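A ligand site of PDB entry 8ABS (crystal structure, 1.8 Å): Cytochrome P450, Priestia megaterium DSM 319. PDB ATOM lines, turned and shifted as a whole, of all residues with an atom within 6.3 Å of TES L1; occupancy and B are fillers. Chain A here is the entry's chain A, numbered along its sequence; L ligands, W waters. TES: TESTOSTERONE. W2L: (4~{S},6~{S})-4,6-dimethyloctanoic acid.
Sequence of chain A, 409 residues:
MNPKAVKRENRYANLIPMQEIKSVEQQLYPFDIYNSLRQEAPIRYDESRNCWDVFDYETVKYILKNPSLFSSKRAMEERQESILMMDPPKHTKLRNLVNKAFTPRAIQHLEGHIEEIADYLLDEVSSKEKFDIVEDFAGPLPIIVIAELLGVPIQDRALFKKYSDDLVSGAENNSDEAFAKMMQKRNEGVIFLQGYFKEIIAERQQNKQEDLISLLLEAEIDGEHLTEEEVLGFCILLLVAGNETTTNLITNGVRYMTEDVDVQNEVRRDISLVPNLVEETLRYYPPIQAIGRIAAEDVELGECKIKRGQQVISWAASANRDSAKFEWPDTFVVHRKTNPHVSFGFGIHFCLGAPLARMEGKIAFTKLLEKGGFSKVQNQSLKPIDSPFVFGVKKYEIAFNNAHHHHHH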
ATOM      1  N   ALA A  75     -31.799  33.002  27.519  1.00  0.00           N
ATOM      2  CA  ALA A  75     -31.871  32.190  26.307  1.00  0.00           C
ATOM      3  C   ALA A  75     -32.483  32.988  25.163  1.00  0.00           C
ATOM      4  O   ALA A  75     -33.420  33.784  25.372  1.00  0.00           O
ATOM      5  CB  ALA A  75     -32.699  30.938  26.583  1.00  0.00           C
ATOM      6  N   GLU A  77     -33.985  31.394  22.678  1.00  0.00           N
ATOM      7  CA  GLU A  77     -35.264  30.710  22.604  1.00  0.00           C
ATOM      8  C   GLU A  77     -36.177  31.192  23.733  1.00  0.00           C
ATOM      9  O   GLU A  77     -35.742  31.839  24.690  1.00  0.00           O
ATOM     10  CB  GLU A  77     -35.063  29.197  22.667  1.00  0.00           C
ATOM     11  CG  GLU A  77     -34.324  28.693  23.909  1.00  0.00           C
ATOM     12  CD  GLU A  77     -32.807  28.661  23.733  1.00  0.00           C
ATOM     13  OE1 GLU A  77     -32.287  29.412  22.879  1.00  0.00           O
ATOM     14  OE2 GLU A  77     -32.144  27.901  24.461  1.00  0.00           O
ATOM     15  N   ARG A  79     -37.745  29.355  25.950  1.00  0.00           N
ATOM     16  CA  ARG A  79     -37.622  28.548  27.159  1.00  0.00           C
ATOM     17  C   ARG A  79     -36.200  28.582  27.693  1.00  0.00           C
ATOM     18  O   ARG A  79     -35.240  28.323  26.965  1.00  0.00           O
ATOM     19  CB  ARG A  79     -38.024  27.097  26.889  1.00  0.00           C
ATOM     20  CG  ARG A  79     -39.460  26.915  26.424  1.00  0.00           C
ATOM     21  CD  ARG A  79     -40.458  27.184  27.546  1.00  0.00           C
ATOM     22  NE  ARG A  79     -41.834  26.989  27.097  1.00  0.00           N
ATOM     23  CZ  ARG A  79     -42.614  27.952  26.632  1.00  0.00           C
ATOM     24  NH1 ARG A  79     -42.200  29.202  26.528  1.00  0.00           N
ATOM     25  NH2 ARG A  79     -43.850  27.650  26.228  1.00  0.00           N
ATOM     26  N   GLU A  81     -33.780  26.576  29.799  1.00  0.00           N
ATOM     27  CA  GLU A  81     -33.910  25.120  29.796  1.00  0.00           C
ATOM     28  C   GLU A  81     -33.250  24.432  30.986  1.00  0.00           C
ATOM     29  O   GLU A  81     -33.794  23.437  31.489  1.00  0.00           O
ATOM     30  CB  GLU A  81     -33.320  24.577  28.487  1.00  0.00           C
ATOM     31  CG  GLU A  81     -33.815  25.327  27.249  1.00  0.00           C
ATOM     32  CD  GLU A  81     -34.609  24.453  26.277  1.00  0.00           C
ATOM     33  OE1 GLU A  81     -35.091  23.372  26.683  1.00  0.00           O
ATOM     34  OE2 GLU A  81     -34.744  24.855  25.103  1.00  0.00           O
ATOM     35  N   SER A  82     -32.105  24.923  31.450  1.00  0.00           N
ATOM     36  CA  SER A  82     -31.357  24.358  32.559  1.00  0.00           C
ATOM     37  C   SER A  82     -31.246  25.406  33.669  1.00  0.00           C
ATOM     38  O   SER A  82     -31.577  26.574  33.456  1.00  0.00           O
ATOM     39  CB  SER A  82     -29.945  23.951  32.133  1.00  0.00           C
ATOM     40  OG  SER A  82     -29.184  25.144  31.933  1.00  0.00           O
ATOM     41  N   LEU A  84     -28.776  26.955  34.659  1.00  0.00           N
ATOM     42  CA  LEU A  84     -27.941  28.093  34.252  1.00  0.00           C
ATOM     43  C   LEU A  84     -28.791  29.281  33.840  1.00  0.00           C
ATOM     44  O   LEU A  84     -28.404  30.439  34.057  1.00  0.00           O
ATOM     45  CB  LEU A  84     -27.047  27.676  33.082  1.00  0.00           C
ATOM     46  CG  LEU A  84     -26.139  28.763  32.529  1.00  0.00           C
ATOM     47  CD1 LEU A  84     -25.129  29.188  33.571  1.00  0.00           C
ATOM     48  CD2 LEU A  84     -25.441  28.291  31.263  1.00  0.00           C
ATOM     49  N   MET A  85     -29.959  29.015  33.262  1.00  0.00           N
ATOM     50  CA  MET A  85     -30.816  30.041  32.686  1.00  0.00           C
ATOM     51  C   MET A  85     -32.061  30.289  33.504  1.00  0.00           C
ATOM     52  O   MET A  85     -33.027  30.865  33.018  1.00  0.00           O
ATOM     53  CB  MET A  85     -31.215  29.628  31.263  1.00  0.00           C
ATOM     54  CG  MET A  85     -30.040  29.246  30.397  1.00  0.00           C
ATOM     55  SD  MET A  85     -29.314  30.723  29.660  1.00  0.00           S
ATOM     56  CE  MET A  85     -27.851  30.041  28.863  1.00  0.00           C
ATOM     57  N   LEU A 167     -21.778  23.718  21.076  1.00  0.00           N
ATOM     58  CA  LEU A 167     -22.758  24.379  21.931  1.00  0.00           C
ATOM     59  C   LEU A 167     -22.207  25.593  22.660  1.00  0.00           C
ATOM     60  O   LEU A 167     -22.984  26.287  23.331  1.00  0.00           O
ATOM     61  CB  LEU A 167     -23.325  23.401  22.944  1.00  0.00           C
ATOM     62  CG  LEU A 167     -24.160  22.257  22.361  1.00  0.00           C
ATOM     63  CD1 LEU A 167     -24.871  21.531  23.500  1.00  0.00           C
ATOM     64  CD2 LEU A 167     -25.148  22.775  21.343  1.00  0.00           C
ATOM     65  N   VAL A 168     -20.903  25.857  22.608  1.00  0.00           N
ATOM     66  CA  VAL A 168     -20.347  27.113  23.125  1.00  0.00           C
ATOM     67  C   VAL A 168     -19.835  28.006  22.018  1.00  0.00           C
ATOM     68  O   VAL A 168     -19.281  29.079  22.312  1.00  0.00           O
ATOM     69  CB  VAL A 168     -19.226  26.874  24.164  1.00  0.00           C
ATOM     70  CG1 VAL A 168     -19.723  25.968  25.299  1.00  0.00           C
ATOM     71  CG2 VAL A 168     -17.990  26.306  23.497  1.00  0.00           C
ATOM     72  N   ARG A 186     -24.557  25.374  16.373  1.00  0.00           N
ATOM     73  CA  ARG A 186     -25.185  25.042  17.652  1.00  0.00           C
ATOM     74  C   ARG A 186     -26.343  24.087  17.434  1.00  0.00           C
ATOM     75  O   ARG A 186     -26.547  23.160  18.234  1.00  0.00           O
ATOM     76  CB  ARG A 186     -25.632  26.320  18.366  1.00  0.00           C
ATOM     77  CG  ARG A 186     -24.438  27.231  18.693  1.00  0.00           C
ATOM     78  CD  ARG A 186     -24.847  28.598  19.260  1.00  0.00           C
ATOM     79  NE  ARG A 186     -25.362  28.477  20.619  1.00  0.00           N
ATOM     80  CZ  ARG A 186     -24.667  28.733  21.721  1.00  0.00           C
ATOM     81  NH1 ARG A 186     -23.410  29.141  21.687  1.00  0.00           N
ATOM     82  NH2 ARG A 186     -25.253  28.565  22.900  1.00  0.00           N
ATOM     83  N   VAL A 190     -27.069  20.437  19.181  1.00  0.00           N
ATOM     84  CA  VAL A 190     -28.321  20.162  19.865  1.00  0.00           C
ATOM     85  C   VAL A 190     -28.951  18.887  19.326  1.00  0.00           C
ATOM     86  O   VAL A 190     -29.463  18.050  20.107  1.00  0.00           O
ATOM     87  CB  VAL A 190     -29.281  21.351  19.715  1.00  0.00           C
ATOM     88  CG1 VAL A 190     -30.671  20.966  20.234  1.00  0.00           C
ATOM     89  CG2 VAL A 190     -28.719  22.575  20.453  1.00  0.00           C
ATOM     90  N   GLN A 194     -28.959  16.288  22.325  1.00  0.00           N
ATOM     91  CA  GLN A 194     -30.312  16.113  22.825  1.00  0.00           C
ATOM     92  C   GLN A 194     -30.857  14.746  22.461  1.00  0.00           C
ATOM     93  O   GLN A 194     -31.466  14.062  23.302  1.00  0.00           O
ATOM     94  CB  GLN A 194     -31.225  17.194  22.294  1.00  0.00           C
ATOM     95  CG  GLN A 194     -32.474  17.385  23.076  1.00  0.00           C
ATOM     96  CD  GLN A 194     -33.311  18.506  22.499  1.00  0.00           C
ATOM     97  OE1 GLN A 194     -34.073  18.303  21.556  1.00  0.00           O
ATOM     98  NE2 GLN A 194     -33.145  19.697  23.051  1.00  0.00           N
ATOM     99  N   GLU A 229     -37.777  17.714  29.600  1.00  0.00           N
ATOM    100  CA  GLU A 229     -36.953  18.866  29.256  1.00  0.00           C
ATOM    101  C   GLU A 229     -36.042  19.231  30.405  1.00  0.00           C
ATOM    102  O   GLU A 229     -34.882  19.639  30.186  1.00  0.00           O
ATOM    103  CB  GLU A 229     -37.854  20.047  28.859  1.00  0.00           C
ATOM    104  CG  GLU A 229     -37.348  21.417  29.301  1.00  0.00           C
ATOM    105  CD  GLU A 229     -38.195  22.585  28.774  1.00  0.00           C
ATOM    106  OE1 GLU A 229     -39.175  22.338  28.046  1.00  0.00           O
ATOM    107  OE2 GLU A 229     -37.871  23.741  29.104  1.00  0.00           O
ATOM    108  N   LEU A 232     -33.158  16.678  30.611  1.00  0.00           N
ATOM    109  CA  LEU A 232     -32.255  16.952  29.499  1.00  0.00           C
ATOM    110  C   LEU A 232     -31.399  18.186  29.749  1.00  0.00           C
ATOM    111  O   LEU A 232     -30.209  18.212  29.404  1.00  0.00           O
ATOM    112  CB  LEU A 232     -33.049  17.172  28.212  1.00  0.00           C
ATOM    113  CG  LEU A 232     -33.406  15.962  27.370  1.00  0.00           C
ATOM    114  CD1 LEU A 232     -34.429  16.398  26.328  1.00  0.00           C
ATOM    115  CD2 LEU A 232     -32.144  15.407  26.714  1.00  0.00           C
ATOM    116  N   GLY A 233     -31.999  19.238  30.318  1.00  0.00           N
ATOM    117  CA  GLY A 233     -31.223  20.424  30.593  1.00  0.00           C
ATOM    118  C   GLY A 233     -30.060  20.157  31.510  1.00  0.00           C
ATOM    119  O   GLY A 233     -28.956  20.641  31.295  1.00  0.00           O
ATOM    120  N   PHE A 234     -30.286  19.335  32.534  1.00  0.00           N
ATOM    121  CA  PHE A 234     -29.212  18.957  33.445  1.00  0.00           C
ATOM    122  C   PHE A 234     -28.131  18.191  32.713  1.00  0.00           C
ATOM    123  O   PHE A 234     -26.933  18.472  32.850  1.00  0.00           O
ATOM    124  CB  PHE A 234     -29.762  18.091  34.572  1.00  0.00           C
ATOM    125  CG  PHE A 234     -30.126  18.846  35.813  1.00  0.00           C
ATOM    126  CD1 PHE A 234     -29.151  19.476  36.572  1.00  0.00           C
ATOM    127  CD2 PHE A 234     -31.446  18.895  36.230  1.00  0.00           C
ATOM    128  CE1 PHE A 234     -29.498  20.165  37.740  1.00  0.00           C
ATOM    129  CE2 PHE A 234     -31.789  19.597  37.402  1.00  0.00           C
ATOM    130  CZ  PHE A 234     -30.804  20.222  38.142  1.00  0.00           C
ATOM    131  N   ILE A 236     -27.256  18.040  29.499  1.00  0.00           N
ATOM    132  CA  ILE A 236     -26.460  18.767  28.526  1.00  0.00           C
ATOM    133  C   ILE A 236     -25.642  19.847  29.205  1.00  0.00           C
ATOM    134  O   ILE A 236     -24.463  20.021  28.886  1.00  0.00           O
ATOM    135  CB  ILE A 236     -27.365  19.317  27.407  1.00  0.00           C
ATOM    136  CG1 ILE A 236     -27.931  18.135  26.609  1.00  0.00           C
ATOM    137  CG2 ILE A 236     -26.613  20.270  26.507  1.00  0.00           C
ATOM    138  CD1 ILE A 236     -29.126  18.460  25.780  1.00  0.00           C
ATOM    139  N   LEU A 237     -26.229  20.554  30.183  1.00  0.00           N
ATOM    140  CA  LEU A 237     -25.453  21.549  30.901  1.00  0.00           C
ATOM    141  C   LEU A 237     -24.261  20.912  31.605  1.00  0.00           C
ATOM    142  O   LEU A 237     -23.134  21.398  31.512  1.00  0.00           O
ATOM    143  CB  LEU A 237     -26.338  22.286  31.920  1.00  0.00           C
ATOM    144  CG  LEU A 237     -25.565  23.195  32.872  1.00  0.00           C
ATOM    145  CD1 LEU A 237     -24.816  24.285  32.151  1.00  0.00           C
ATOM    146  CD2 LEU A 237     -26.553  23.803  33.855  1.00  0.00           C
ATOM    147  N   VAL A 240     -21.540  19.778  29.013  1.00  0.00           N
ATOM    148  CA  VAL A 240     -20.799  20.827  28.334  1.00  0.00           C
ATOM    149  C   VAL A 240     -19.965  21.622  29.326  1.00  0.00           C
ATOM    150  O   VAL A 240     -18.783  21.857  29.104  1.00  0.00           O
ATOM    151  CB  VAL A 240     -21.759  21.737  27.557  1.00  0.00           C
ATOM    152  CG1 VAL A 240     -20.998  22.912  26.995  1.00  0.00           C
ATOM    153  CG2 VAL A 240     -22.435  20.955  26.436  1.00  0.00           C
ATOM    154  N   ALA A 241     -20.581  22.068  30.429  1.00  0.00           N
ATOM    155  CA  ALA A 241     -19.833  22.785  31.454  1.00  0.00           C
ATOM    156  C   ALA A 241     -18.756  21.887  32.064  1.00  0.00           C
ATOM    157  O   ALA A 241     -17.656  22.358  32.387  1.00  0.00           O
ATOM    158  CB  ALA A 241     -20.771  23.293  32.542  1.00  0.00           C
ATOM    159  N   PHE A 389     -16.806  34.382  24.543  1.00  0.00           N
ATOM    160  CA  PHE A 389     -16.899  34.259  26.005  1.00  0.00           C
ATOM    161  C   PHE A 389     -16.048  33.133  26.538  1.00  0.00           C
ATOM    162  O   PHE A 389     -15.989  32.924  27.750  1.00  0.00           O
ATOM    163  CB  PHE A 389     -18.359  34.101  26.446  1.00  0.00           C
ATOM    164  CG  PHE A 389     -18.946  32.731  26.200  1.00  0.00           C
ATOM    165  CD1 PHE A 389     -18.899  31.766  27.195  1.00  0.00           C
ATOM    166  CD2 PHE A 389     -19.597  32.446  25.030  1.00  0.00           C
ATOM    167  CE1 PHE A 389     -19.460  30.531  27.009  1.00  0.00           C
ATOM    168  CE2 PHE A 389     -20.151  31.194  24.821  1.00  0.00           C
ATOM    169  CZ  PHE A 389     -20.079  30.241  25.828  1.00  0.00           C
HETATM  170  C1  TES L   1     -30.199  23.329  24.577  1.00  0.00           C
HETATM  171  C2  TES L   1     -30.337  21.818  24.587  1.00  0.00           C
HETATM  172  C3  TES L   1     -31.185  21.364  25.737  1.00  0.00           C
HETATM  173  O3  TES L   1     -32.012  20.469  25.651  1.00  0.00           O
HETATM  174  C4  TES L   1     -30.944  22.112  26.960  1.00  0.00           C
HETATM  175  C5  TES L   1     -30.003  23.052  27.046  1.00  0.00           C
HETATM  176  C6  TES L   1     -29.548  23.445  28.410  1.00  0.00           C
HETATM  177  C7  TES L   1     -28.026  23.591  28.372  1.00  0.00           C
HETATM  178  C8  TES L   1     -27.627  24.639  27.332  1.00  0.00           C
HETATM  179  C9  TES L   1     -28.123  24.227  25.918  1.00  0.00           C
HETATM  180  C10 TES L   1     -29.663  23.977  25.888  1.00  0.00           C
HETATM  181  C11 TES L   1     -27.602  25.228  24.874  1.00  0.00           C
HETATM  182  C12 TES L   1     -26.083  25.457  24.939  1.00  0.00           C
HETATM  183  C13 TES L   1     -25.626  25.883  26.344  1.00  0.00           C
HETATM  184  C14 TES L   1     -26.129  24.830  27.343  1.00  0.00           C
HETATM  185  C15 TES L   1     -25.422  25.210  28.651  1.00  0.00           C
HETATM  186  C16 TES L   1     -24.004  25.586  28.160  1.00  0.00           C
HETATM  187  C17 TES L   1     -24.130  25.788  26.636  1.00  0.00           C
HETATM  188  O17 TES L   1     -23.428  26.930  26.159  1.00  0.00           O
HETATM  189  C18 TES L   1     -26.152  27.294  26.674  1.00  0.00           C
HETATM  190  C19 TES L   1     -30.452  25.274  26.006  1.00  0.00           C
HETATM  191  CAA W2L L   2     -20.577  26.341  30.149  1.00  0.00           C
HETATM  192  CAB W2L L   2     -19.886  26.983  31.265  1.00  0.00           C
HETATM  193  CAC W2L L   2     -20.866  27.767  32.169  1.00  0.00           C
HETATM  194  CAD W2L L   2     -22.064  26.991  32.643  1.00  0.00           C
HETATM  195  CAE W2L L   2     -21.500  28.915  31.347  1.00  0.00           C
HETATM  196  CAF W2L L   2     -21.296  30.223  32.081  1.00  0.00           C
HETATM  197  CAG W2L L   2     -19.824  30.403  32.027  1.00  0.00           C
HETATM  198  CAH W2L L   2     -22.201  31.396  31.469  1.00  0.00           C
HETATM  199  CAI W2L L   2     -21.759  31.694  30.095  1.00  0.00           C
HETATM  200  CAJ W2L L   2     -22.684  32.882  29.699  1.00  0.00           C
HETATM  201  OAK W2L L   2     -23.042  33.670  30.607  1.00  0.00           O
HETATM  202  OAL W2L L   2     -23.021  32.964  28.500  1.00  0.00           O
HETATM  203  O   HOH W   1     -23.510  29.178  25.055  1.00  0.00           O
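Water W1 lies within hydrogen-bond range of O17 of TES L1, NH2 of Arg 186 and O of Leu 167.
The side-chain hydroxyl (OG) of Ser 82 sits close to the backbone NH (N) of Leu 84 (3.3 Å). The guanidinium group (NH2) of Arg 186 lies within hydrogen-bond range of the backbone carbonyl oxygen (O) of Leu 167, 3.2 Å away.
Glu 77 touches TES L1. Glu 81 touches TES L1. CB of Ser 82 touches C6 of TES L1 (3.8 Å). CE of Met 85 touches C18 of TES L1, at 3.9 Å. Val 168 touches TES L1. Arg 186 touches TES L1 (NH2 to C12, 3.8 Å). Ile 236 touches TES L1. CD1 of Leu 237 touches C15 of TES L1 (3.7 Å).
The side-chain amide nitrogen (NE2) of Gln 194 is in hydrogen-bond range of an oxygen (O3) of TES L1 (2.9 Å). O17 of TES L1 is in hydrogen-bond range of O of Leu 167 (2.9 Å).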
